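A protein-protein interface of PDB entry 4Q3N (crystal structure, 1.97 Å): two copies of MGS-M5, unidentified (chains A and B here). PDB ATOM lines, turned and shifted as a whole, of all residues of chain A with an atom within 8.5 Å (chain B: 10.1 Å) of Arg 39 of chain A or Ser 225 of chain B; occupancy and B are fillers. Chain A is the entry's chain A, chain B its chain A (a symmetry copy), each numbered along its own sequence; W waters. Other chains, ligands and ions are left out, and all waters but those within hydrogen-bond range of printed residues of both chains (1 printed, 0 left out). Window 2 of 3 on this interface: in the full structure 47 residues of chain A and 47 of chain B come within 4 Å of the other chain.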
ATOM      1  N   THR A  11     -13.477   4.785 -20.820  1.00  0.00           N
ATOM      2  CA  THR A  11     -12.378   5.367 -21.591  1.00  0.00           C
ATOM      3  C   THR A  11     -11.768   6.583 -20.836  1.00  0.00           C
ATOM      4  O   THR A  11     -11.612   7.644 -21.401  1.00  0.00           O
ATOM      5  CB  THR A  11     -12.854   5.780 -23.021  1.00  0.00           C
ATOM      6  OG1 THR A  11     -13.958   6.674 -22.915  1.00  0.00           O
ATOM      7  CG2 THR A  11     -13.297   4.590 -23.856  1.00  0.00           C
ATOM      8  N   ASP A  35     -18.017   3.223 -23.342  1.00  0.00           N
ATOM      9  CA  ASP A  35     -18.072   4.198 -22.273  1.00  0.00           C
ATOM     10  C   ASP A  35     -19.510   4.603 -22.098  1.00  0.00           C
ATOM     11  O   ASP A  35     -20.256   4.649 -23.072  1.00  0.00           O
ATOM     12  CB  ASP A  35     -17.215   5.428 -22.595  1.00  0.00           C
ATOM     13  CG  ASP A  35     -16.948   6.279 -21.373  1.00  0.00           C
ATOM     14  OD1 ASP A  35     -17.815   7.097 -21.015  1.00  0.00           O
ATOM     15  OD2 ASP A  35     -15.890   6.139 -20.759  1.00  0.00           O
ATOM     16  N   ILE A  36     -19.914   4.906 -20.877  1.00  0.00           N
ATOM     17  CA  ILE A  36     -21.289   5.380 -20.675  1.00  0.00           C
ATOM     18  C   ILE A  36     -21.502   6.666 -21.484  1.00  0.00           C
ATOM     19  O   ILE A  36     -22.606   6.982 -21.891  1.00  0.00           O
ATOM     20  CB  ILE A  36     -21.579   5.580 -19.178  1.00  0.00           C
ATOM     21  CG1 ILE A  36     -22.987   6.119 -18.996  1.00  0.00           C
ATOM     22  CG2 ILE A  36     -20.557   6.486 -18.548  1.00  0.00           C
ATOM     23  CD1 ILE A  36     -24.067   5.247 -19.678  1.00  0.00           C
ATOM     24  N   ASP A  37     -20.441   7.406 -21.762  1.00  0.00           N
ATOM     25  CA  ASP A  37     -20.561   8.614 -22.601  1.00  0.00           C
ATOM     26  C   ASP A  37     -20.193   8.151 -24.015  1.00  0.00           C
ATOM     27  O   ASP A  37     -19.000   8.033 -24.351  1.00  0.00           O
ATOM     28  CB  ASP A  37     -19.633   9.733 -22.079  1.00  0.00           C
ATOM     29  CG  ASP A  37     -19.624  10.985 -22.962  1.00  0.00           C
ATOM     30  OD1 ASP A  37     -20.231  10.995 -24.048  1.00  0.00           O
ATOM     31  OD2 ASP A  37     -18.995  11.986 -22.552  1.00  0.00           O
ATOM     32  N   LYS A  38     -21.196   7.838 -24.832  1.00  0.00           N
ATOM     33  CA  LYS A  38     -20.912   7.218 -26.136  1.00  0.00           C
ATOM     34  C   LYS A  38     -20.120   8.158 -27.056  1.00  0.00           C
ATOM     35  O   LYS A  38     -19.250   7.699 -27.761  1.00  0.00           O
ATOM     36  CB  LYS A  38     -22.206   6.793 -26.846  1.00  0.00           C
ATOM     37  CG  LYS A  38     -22.033   6.166 -28.273  1.00  0.00           C
ATOM     38  CD  LYS A  38     -21.051   4.972 -28.385  1.00  0.00           C
ATOM     39  CE  LYS A  38     -21.120   4.287 -29.792  1.00  0.00           C
ATOM     40  NZ  LYS A  38     -22.245   3.303 -29.929  1.00  0.00           N
ATOM     41  N   ARG A  39     -20.461   9.449 -27.041  1.00  0.00           N
ATOM     42  CA  ARG A  39     -19.773  10.452 -27.850  1.00  0.00           C
ATOM     43  C   ARG A  39     -18.288  10.505 -27.516  1.00  0.00           C
ATOM     44  O   ARG A  39     -17.441  10.672 -28.403  1.00  0.00           O
ATOM     45  CB  ARG A  39     -20.389  11.841 -27.639  1.00  0.00           C
ATOM     46  CG  ARG A  39     -21.711  12.053 -28.342  1.00  0.00           C
ATOM     47  CD  ARG A  39     -22.217  13.484 -28.153  1.00  0.00           C
ATOM     48  NE  ARG A  39     -21.367  14.486 -28.808  1.00  0.00           N
ATOM     49  CZ  ARG A  39     -20.483  15.268 -28.187  1.00  0.00           C
ATOM     50  NH1 ARG A  39     -20.305  15.195 -26.865  1.00  0.00           N
ATOM     51  NH2 ARG A  39     -19.784  16.140 -28.900  1.00  0.00           N
ATOM     52  N   LYS A  40     -17.982  10.399 -26.226  1.00  0.00           N
ATOM     53  CA  LYS A  40     -16.598  10.403 -25.784  1.00  0.00           C
ATOM     54  C   LYS A  40     -15.861   9.165 -26.353  1.00  0.00           C
ATOM     55  O   LYS A  40     -14.757   9.279 -26.926  1.00  0.00           O
ATOM     56  CB  LYS A  40     -16.557  10.450 -24.262  1.00  0.00           C
ATOM     57  CG  LYS A  40     -15.296   9.941 -23.600  1.00  0.00           C
ATOM     58  CD  LYS A  40     -14.260  10.989 -23.375  1.00  0.00           C
ATOM     59  CE  LYS A  40     -13.382  10.628 -22.172  1.00  0.00           C
ATOM     60  NZ  LYS A  40     -11.988  10.230 -22.578  1.00  0.00           N
ATOM     61  N   ALA A  41     -16.460   7.983 -26.231  1.00  0.00           N
ATOM     62  CA  ALA A  41     -15.815   6.795 -26.775  1.00  0.00           C
ATOM     63  C   ALA A  41     -15.583   6.917 -28.288  1.00  0.00           C
ATOM     64  O   ALA A  41     -14.563   6.450 -28.810  1.00  0.00           O
ATOM     65  CB  ALA A  41     -16.644   5.531 -26.458  1.00  0.00           C
ATOM     66  N   GLU A  42     -16.559   7.477 -28.993  1.00  0.00           N
ATOM     67  CA  GLU A  42     -16.414   7.730 -30.421  1.00  0.00           C
ATOM     68  C   GLU A  42     -15.251   8.679 -30.734  1.00  0.00           C
ATOM     69  O   GLU A  42     -14.530   8.467 -31.713  1.00  0.00           O
ATOM     70  CB  GLU A  42     -17.741   8.322 -30.995  1.00  0.00           C
ATOM     71  CG  GLU A  42     -18.796   7.237 -31.003  1.00  0.00           C
ATOM     72  CD  GLU A  42     -20.177   7.719 -31.400  1.00  0.00           C
ATOM     73  OE1 GLU A  42     -21.028   6.852 -31.709  1.00  0.00           O
ATOM     74  OE2 GLU A  42     -20.408   8.940 -31.385  1.00  0.00           O
ATOM     75  N   GLY A  43     -15.099   9.738 -29.935  1.00  0.00           N
ATOM     76  CA  GLY A  43     -13.971  10.661 -30.100  1.00  0.00           C
ATOM     77  C   GLY A  43     -12.648   9.977 -29.858  1.00  0.00           C
ATOM     78  O   GLY A  43     -11.661  10.225 -30.573  1.00  0.00           O
ATOM     79  N   GLU A  44     -12.608   9.096 -28.862  1.00  0.00           N
ATOM     80  CA  GLU A  44     -11.372   8.390 -28.542  1.00  0.00           C
ATOM     81  C   GLU A  44     -11.035   7.431 -29.680  1.00  0.00           C
ATOM     82  O   GLU A  44      -9.887   7.284 -30.053  1.00  0.00           O
ATOM     83  CB  GLU A  44     -11.494   7.598 -27.215  1.00  0.00           C
ATOM     84  CG  GLU A  44     -11.610   8.504 -25.960  1.00  0.00           C
ATOM     85  CD  GLU A  44     -10.286   9.180 -25.609  1.00  0.00           C
ATOM     86  OE1 GLU A  44      -9.321   9.083 -26.430  1.00  0.00           O
ATOM     87  OE2 GLU A  44     -10.207   9.855 -24.545  1.00  0.00           O
ATOM     88  N   ALA A  45     -12.041   6.759 -30.218  1.00  0.00           N
ATOM     89  CA  ALA A  45     -11.766   5.859 -31.377  1.00  0.00           C
ATOM     90  C   ALA A  45     -11.245   6.664 -32.585  1.00  0.00           C
ATOM     91  O   ALA A  45     -10.314   6.225 -33.254  1.00  0.00           O
ATOM     92  CB  ALA A  45     -13.039   5.084 -31.759  1.00  0.00           C
ATOM     93  N   MET A  46     -11.838   7.834 -32.871  1.00  0.00           N
ATOM     94  CA  MET A  46     -11.297   8.688 -33.955  1.00  0.00           C
ATOM     95  C   MET A  46      -9.819   8.975 -33.701  1.00  0.00           C
ATOM     96  O   MET A  46      -8.967   8.781 -34.583  1.00  0.00           O
ATOM     97  CB  MET A  46     -12.033  10.002 -34.071  1.00  0.00           C
ATOM     98  CG  MET A  46     -13.483   9.871 -34.454  1.00  0.00           C
ATOM     99  SD  MET A  46     -14.305  11.444 -34.216  1.00  0.00           S
ATOM    100  CE  MET A  46     -15.995  10.971 -34.675  1.00  0.00           C
ATOM    101  N   ALA A  63     -15.812   2.633 -31.385  1.00  0.00           N
ATOM    102  CA  ALA A  63     -16.574   2.701 -30.136  1.00  0.00           C
ATOM    103  C   ALA A  63     -17.690   1.689 -30.286  1.00  0.00           C
ATOM    104  O   ALA A  63     -18.239   1.580 -31.369  1.00  0.00           O
ATOM    105  CB  ALA A  63     -17.196   4.181 -29.898  1.00  0.00           C
ATOM    106  N   ASP B 218     -12.741  18.735 -40.609  1.00  0.00           N
ATOM    107  CA  ASP B 218     -13.542  18.840 -39.381  1.00  0.00           C
ATOM    108  C   ASP B 218     -13.052  17.905 -38.282  1.00  0.00           C
ATOM    109  O   ASP B 218     -13.577  17.950 -37.175  1.00  0.00           O
ATOM    110  CB  ASP B 218     -14.987  18.493 -39.683  1.00  0.00           C
ATOM    111  CG  ASP B 218     -15.966  19.061 -38.668  1.00  0.00           C
ATOM    112  OD1 ASP B 218     -15.800  20.226 -38.178  1.00  0.00           O
ATOM    113  OD2 ASP B 218     -16.964  18.356 -38.416  1.00  0.00           O
ATOM    114  N   ALA B 219     -12.049  17.069 -38.587  1.00  0.00           N
ATOM    115  CA  ALA B 219     -11.616  16.016 -37.644  1.00  0.00           C
ATOM    116  C   ALA B 219     -11.175  16.515 -36.269  1.00  0.00           C
ATOM    117  O   ALA B 219     -11.616  15.990 -35.248  1.00  0.00           O
ATOM    118  CB  ALA B 219     -10.494  15.172 -38.270  1.00  0.00           C
ATOM    119  N   ALA B 220     -10.323  17.535 -36.220  1.00  0.00           N
ATOM    120  CA  ALA B 220      -9.907  18.083 -34.933  1.00  0.00           C
ATOM    121  C   ALA B 220     -11.084  18.585 -34.121  1.00  0.00           C
ATOM    122  O   ALA B 220     -11.203  18.323 -32.916  1.00  0.00           O
ATOM    123  CB  ALA B 220      -8.911  19.228 -35.139  1.00  0.00           C
ATOM    124  N   TYR B 221     -11.930  19.378 -34.762  1.00  0.00           N
ATOM    125  CA  TYR B 221     -13.099  19.908 -34.060  1.00  0.00           C
ATOM    126  C   TYR B 221     -13.942  18.791 -33.484  1.00  0.00           C
ATOM    127  O   TYR B 221     -14.463  18.862 -32.358  1.00  0.00           O
ATOM    128  CB  TYR B 221     -13.986  20.749 -34.998  1.00  0.00           C
ATOM    129  CG  TYR B 221     -15.197  21.267 -34.275  1.00  0.00           C
ATOM    130  CD1 TYR B 221     -16.343  20.495 -34.142  1.00  0.00           C
ATOM    131  CD2 TYR B 221     -15.196  22.549 -33.729  1.00  0.00           C
ATOM    132  CE1 TYR B 221     -17.473  20.984 -33.440  1.00  0.00           C
ATOM    133  CE2 TYR B 221     -16.299  23.043 -33.057  1.00  0.00           C
ATOM    134  CZ  TYR B 221     -17.435  22.256 -32.915  1.00  0.00           C
ATOM    135  OH  TYR B 221     -18.534  22.752 -32.273  1.00  0.00           O
ATOM    136  N   GLU B 222     -14.124  17.775 -34.307  1.00  0.00           N
ATOM    137  CA  GLU B 222     -14.983  16.656 -33.947  1.00  0.00           C
ATOM    138  C   GLU B 222     -14.433  15.957 -32.681  1.00  0.00           C
ATOM    139  O   GLU B 222     -15.187  15.647 -31.739  1.00  0.00           O
ATOM    140  CB  GLU B 222     -15.059  15.692 -35.146  1.00  0.00           C
ATOM    141  CG  GLU B 222     -16.125  14.670 -35.117  1.00  0.00           C
ATOM    142  CD  GLU B 222     -17.510  15.260 -34.865  1.00  0.00           C
ATOM    143  OE1 GLU B 222     -18.041  15.934 -35.778  1.00  0.00           O
ATOM    144  OE2 GLU B 222     -18.040  15.036 -33.738  1.00  0.00           O
ATOM    145  N   ILE B 223     -13.122  15.722 -32.665  1.00  0.00           N
ATOM    146  CA  ILE B 223     -12.510  15.045 -31.541  1.00  0.00           C
ATOM    147  C   ILE B 223     -12.555  15.946 -30.288  1.00  0.00           C
ATOM    148  O   ILE B 223     -12.984  15.522 -29.220  1.00  0.00           O
ATOM    149  CB  ILE B 223     -11.078  14.619 -31.883  1.00  0.00           C
ATOM    150  CG1 ILE B 223     -11.120  13.435 -32.885  1.00  0.00           C
ATOM    151  CG2 ILE B 223     -10.320  14.142 -30.584  1.00  0.00           C
ATOM    152  CD1 ILE B 223      -9.750  13.231 -33.727  1.00  0.00           C
ATOM    153  N   ILE B 224     -12.140  17.195 -30.443  1.00  0.00           N
ATOM    154  CA  ILE B 224     -12.179  18.163 -29.335  1.00  0.00           C
ATOM    155  C   ILE B 224     -13.549  18.241 -28.734  1.00  0.00           C
ATOM    156  O   ILE B 224     -13.684  18.283 -27.504  1.00  0.00           O
ATOM    157  CB  ILE B 224     -11.747  19.560 -29.821  1.00  0.00           C
ATOM    158  CG1 ILE B 224     -10.236  19.557 -30.149  1.00  0.00           C
ATOM    159  CG2 ILE B 224     -12.078  20.654 -28.776  1.00  0.00           C
ATOM    160  CD1 ILE B 224      -9.832  20.657 -31.129  1.00  0.00           C
ATOM    161  N   SER B 225     -14.590  18.234 -29.574  1.00  0.00           N
ATOM    162  CA  SER B 225     -15.931  18.399 -29.025  1.00  0.00           C
ATOM    163  C   SER B 225     -16.374  17.154 -28.225  1.00  0.00           C
ATOM    164  O   SER B 225     -17.345  17.208 -27.480  1.00  0.00           O
ATOM    165  CB  SER B 225     -16.964  18.674 -30.131  1.00  0.00           C
ATOM    166  OG  SER B 225     -17.146  17.501 -30.928  1.00  0.00           O
ATOM    167  N   ARG B 226     -15.700  16.026 -28.424  1.00  0.00           N
ATOM    168  CA  ARG B 226     -16.101  14.760 -27.787  1.00  0.00           C
ATOM    169  C   ARG B 226     -15.231  14.352 -26.588  1.00  0.00           C
ATOM    170  O   ARG B 226     -15.707  13.713 -25.638  1.00  0.00           O
ATOM    171  CB  ARG B 226     -16.034  13.625 -28.816  1.00  0.00           C
ATOM    172  CG  ARG B 226     -17.189  13.615 -29.748  1.00  0.00           C
ATOM    173  CD  ARG B 226     -16.787  12.785 -30.982  1.00  0.00           C
ATOM    174  NE  ARG B 226     -17.795  12.963 -32.031  1.00  0.00           N
ATOM    175  CZ  ARG B 226     -18.868  12.216 -32.161  1.00  0.00           C
ATOM    176  NH1 ARG B 226     -19.108  11.245 -31.289  1.00  0.00           N
ATOM    177  NH2 ARG B 226     -19.710  12.452 -33.163  1.00  0.00           N
ATOM    178  N   LYS B 227     -13.935  14.660 -26.677  1.00  0.00           N
ATOM    179  CA  LYS B 227     -13.010  14.314 -25.600  1.00  0.00           C
ATOM    180  C   LYS B 227     -12.062  15.468 -25.195  1.00  0.00           C
ATOM    181  O   LYS B 227     -10.974  15.197 -24.715  1.00  0.00           O
ATOM    182  CB  LYS B 227     -12.180  13.079 -26.011  1.00  0.00           C
ATOM    183  CG  LYS B 227     -11.414  13.262 -27.289  1.00  0.00           C
ATOM    184  CD  LYS B 227     -10.337  12.093 -27.472  1.00  0.00           C
ATOM    185  CE  LYS B 227      -9.092  12.367 -26.628  1.00  0.00           C
ATOM    186  NZ  LYS B 227      -7.956  11.421 -26.910  1.00  0.00           N
ATOM    187  N   LYS B 228     -12.471  16.725 -25.425  1.00  0.00           N
ATOM    188  CA  LYS B 228     -11.773  17.962 -24.960  1.00  0.00           C
ATOM    189  C   LYS B 228     -10.546  18.373 -25.748  1.00  0.00           C
ATOM    190  O   LYS B 228     -10.272  19.552 -25.909  1.00  0.00           O
ATOM    191  CB  LYS B 228     -11.377  17.863 -23.472  1.00  0.00           C
ATOM    192  CG  LYS B 228     -12.575  17.782 -22.531  1.00  0.00           C
ATOM    193  CD  LYS B 228     -12.131  17.625 -21.075  1.00  0.00           C
ATOM    194  CE  LYS B 228     -13.315  17.397 -20.151  1.00  0.00           C
ATOM    195  NZ  LYS B 228     -12.900  17.440 -18.701  1.00  0.00           N
ATOM    196  N   ALA B 229      -9.799  17.413 -26.285  1.00  0.00           N
ATOM    197  CA  ALA B 229      -8.565  17.742 -26.964  1.00  0.00           C
ATOM    198  C   ALA B 229      -8.186  16.574 -27.874  1.00  0.00           C
ATOM    199  O   ALA B 229      -8.619  15.458 -27.622  1.00  0.00           O
ATOM    200  CB  ALA B 229      -7.441  18.018 -25.930  1.00  0.00           C
ATOM    201  N   THR B 230      -7.423  16.829 -28.922  1.00  0.00           N
ATOM    202  CA  THR B 230      -6.911  15.717 -29.723  1.00  0.00           C
ATOM    203  C   THR B 230      -5.414  15.552 -29.433  1.00  0.00           C
ATOM    204  O   THR B 230      -4.695  16.549 -29.294  1.00  0.00           O
ATOM    205  CB  THR B 230      -7.203  15.966 -31.230  1.00  0.00           C
ATOM    206  OG1 THR B 230      -6.511  15.003 -32.034  1.00  0.00           O
ATOM    207  CG2 THR B 230      -6.796  17.342 -31.650  1.00  0.00           C
HETATM  208  O   HOH W   1     -18.304  13.725 -24.709  1.00  0.00           O
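No position is printed for both chains.
Of the 12 pairs that touch across the chains among the printed residues, none has its exchanged pair printed and touching as well.
The side-chain carboxylate (OE2) of Glu 42 of chain A is in salt-bridge range of the guanidinium group (NH1) of Arg 226 of chain B, at 2.6 Å.
NH2 of Arg 39 of chain A sits at hydrogen-bond distance from O of Ser 225 of chain B (3.0 Å).
O of Arg 39 of chain A lies close to NH1 of Arg 226 of chain B.
The side-chain carboxylate of Glu 44 of chain A is in salt-bridge range of the side-chain amino group of Lys 227 of chain B (2.7 Å).
Water W1 lies within hydrogen-bond range of the backbone carbonyl oxygen (O) of Arg 226 of chain B (2.8 Å), the side-chain carboxylate (OD2) of Asp 37 of chain A (2.9 Å) and the guanidinium group (NH1) of Arg 39 of chain A (3.3 Å).
The guanidinium group of Arg 226 of chain B lies within salt-bridge range of the side-chain carboxylate of Glu 222 of chain B (2.7 Å).
The backbone carbonyl oxygen of Glu 222 of chain B lies within hydrogen-bond range of the side-chain hydroxyl of Ser 225 of chain B, 2.8 Å away.
The backbone carbonyl oxygen of Tyr 221 of chain B lies within hydrogen-bond range of the side-chain hydroxyl of Ser 225 of chain B.
NZ of Lys 40 of chain A lies within hydrogen-bond range of O of Thr 11 of chain A.
OD1 of Asp 37 of chain A lies close to N of Arg 39 of chain A (3.4 Å).
The side-chain amino group (NZ) of Lys 40 of chain A lies within salt-bridge range of the side-chain carboxylate (OE2) of Glu 44 of chain A.
Among the printed residues, pairs that only touch across the chains: Lys 40 of chain A with Arg 226 of chain B (3.4 Å), Gly 43 of chain A with Arg 226 of chain B (3.6 Å), Met 46 of chain A with Glu 222 of chain B (3.7 Å), Met 46 of chain A with Ile 223 of chain B (3.7 Å), Met 46 of chain A with Arg 226 of chain B (3.8 Å), Gly 43 of chain A with Lys 227 of chain B (3.9 Å), Lys 40 of chain A with Lys 227 of chain B (3.96 Å) and Gly 43 of chain A with Ile 223 of chain B (3.99 Å).
Thr 11 of chain A touches none of the printed residues of chain B.
No residue of chain B comes within 4 Å of Asp 37 of chain A.
Of the printed residues of chain B, Arg 39 of chain A touches Ser 225 and Arg 226.
Printed residues of chain B within 4 Å of Lys 40 of chain A: Arg 226 (3.4 Å) and Lys 227 (3.96 Å).
No residue of chain B comes within 4 Å of Ala 41 of chain A.
Of chain B, only Arg 226 (2.6 Å) comes within 4 Å of Glu 42 of chain A.
Printed residues of chain B within 4 Å of Gly 43 of chain A: Ile 223 (3.99 Å), Arg 226 (3.6 Å) and Lys 227 (3.9 Å).
Printed residues of chain A within 4 Å of Glu 222 of chain B: Met 46 (3.7 Å).
Printed residues of chain A within 4 Å of Ser 225 of chain B: Arg 39.
Of the printed residues of chain A, Arg 226 of chain B touches Arg 39 (3.2 Å), Lys 40 (3.4 Å), Glu 42 (2.6 Å), Gly 43 (3.6 Å) and Met 46 (3.8 Å).
Printed residues of chain A within 4 Å of Lys 227 of chain B: Lys 40, Gly 43 and Glu 44.
Ala 229 of chain B touches none of the printed residues of chain A.
The nearest printed residue of chain B that does not touch Glu 44 of chain A is Arg 226 of chain B (5.7 Å).
Hydrophobic or aromatic side chains of chain B within 4 Å of the printed part of chain A: Ile 223.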
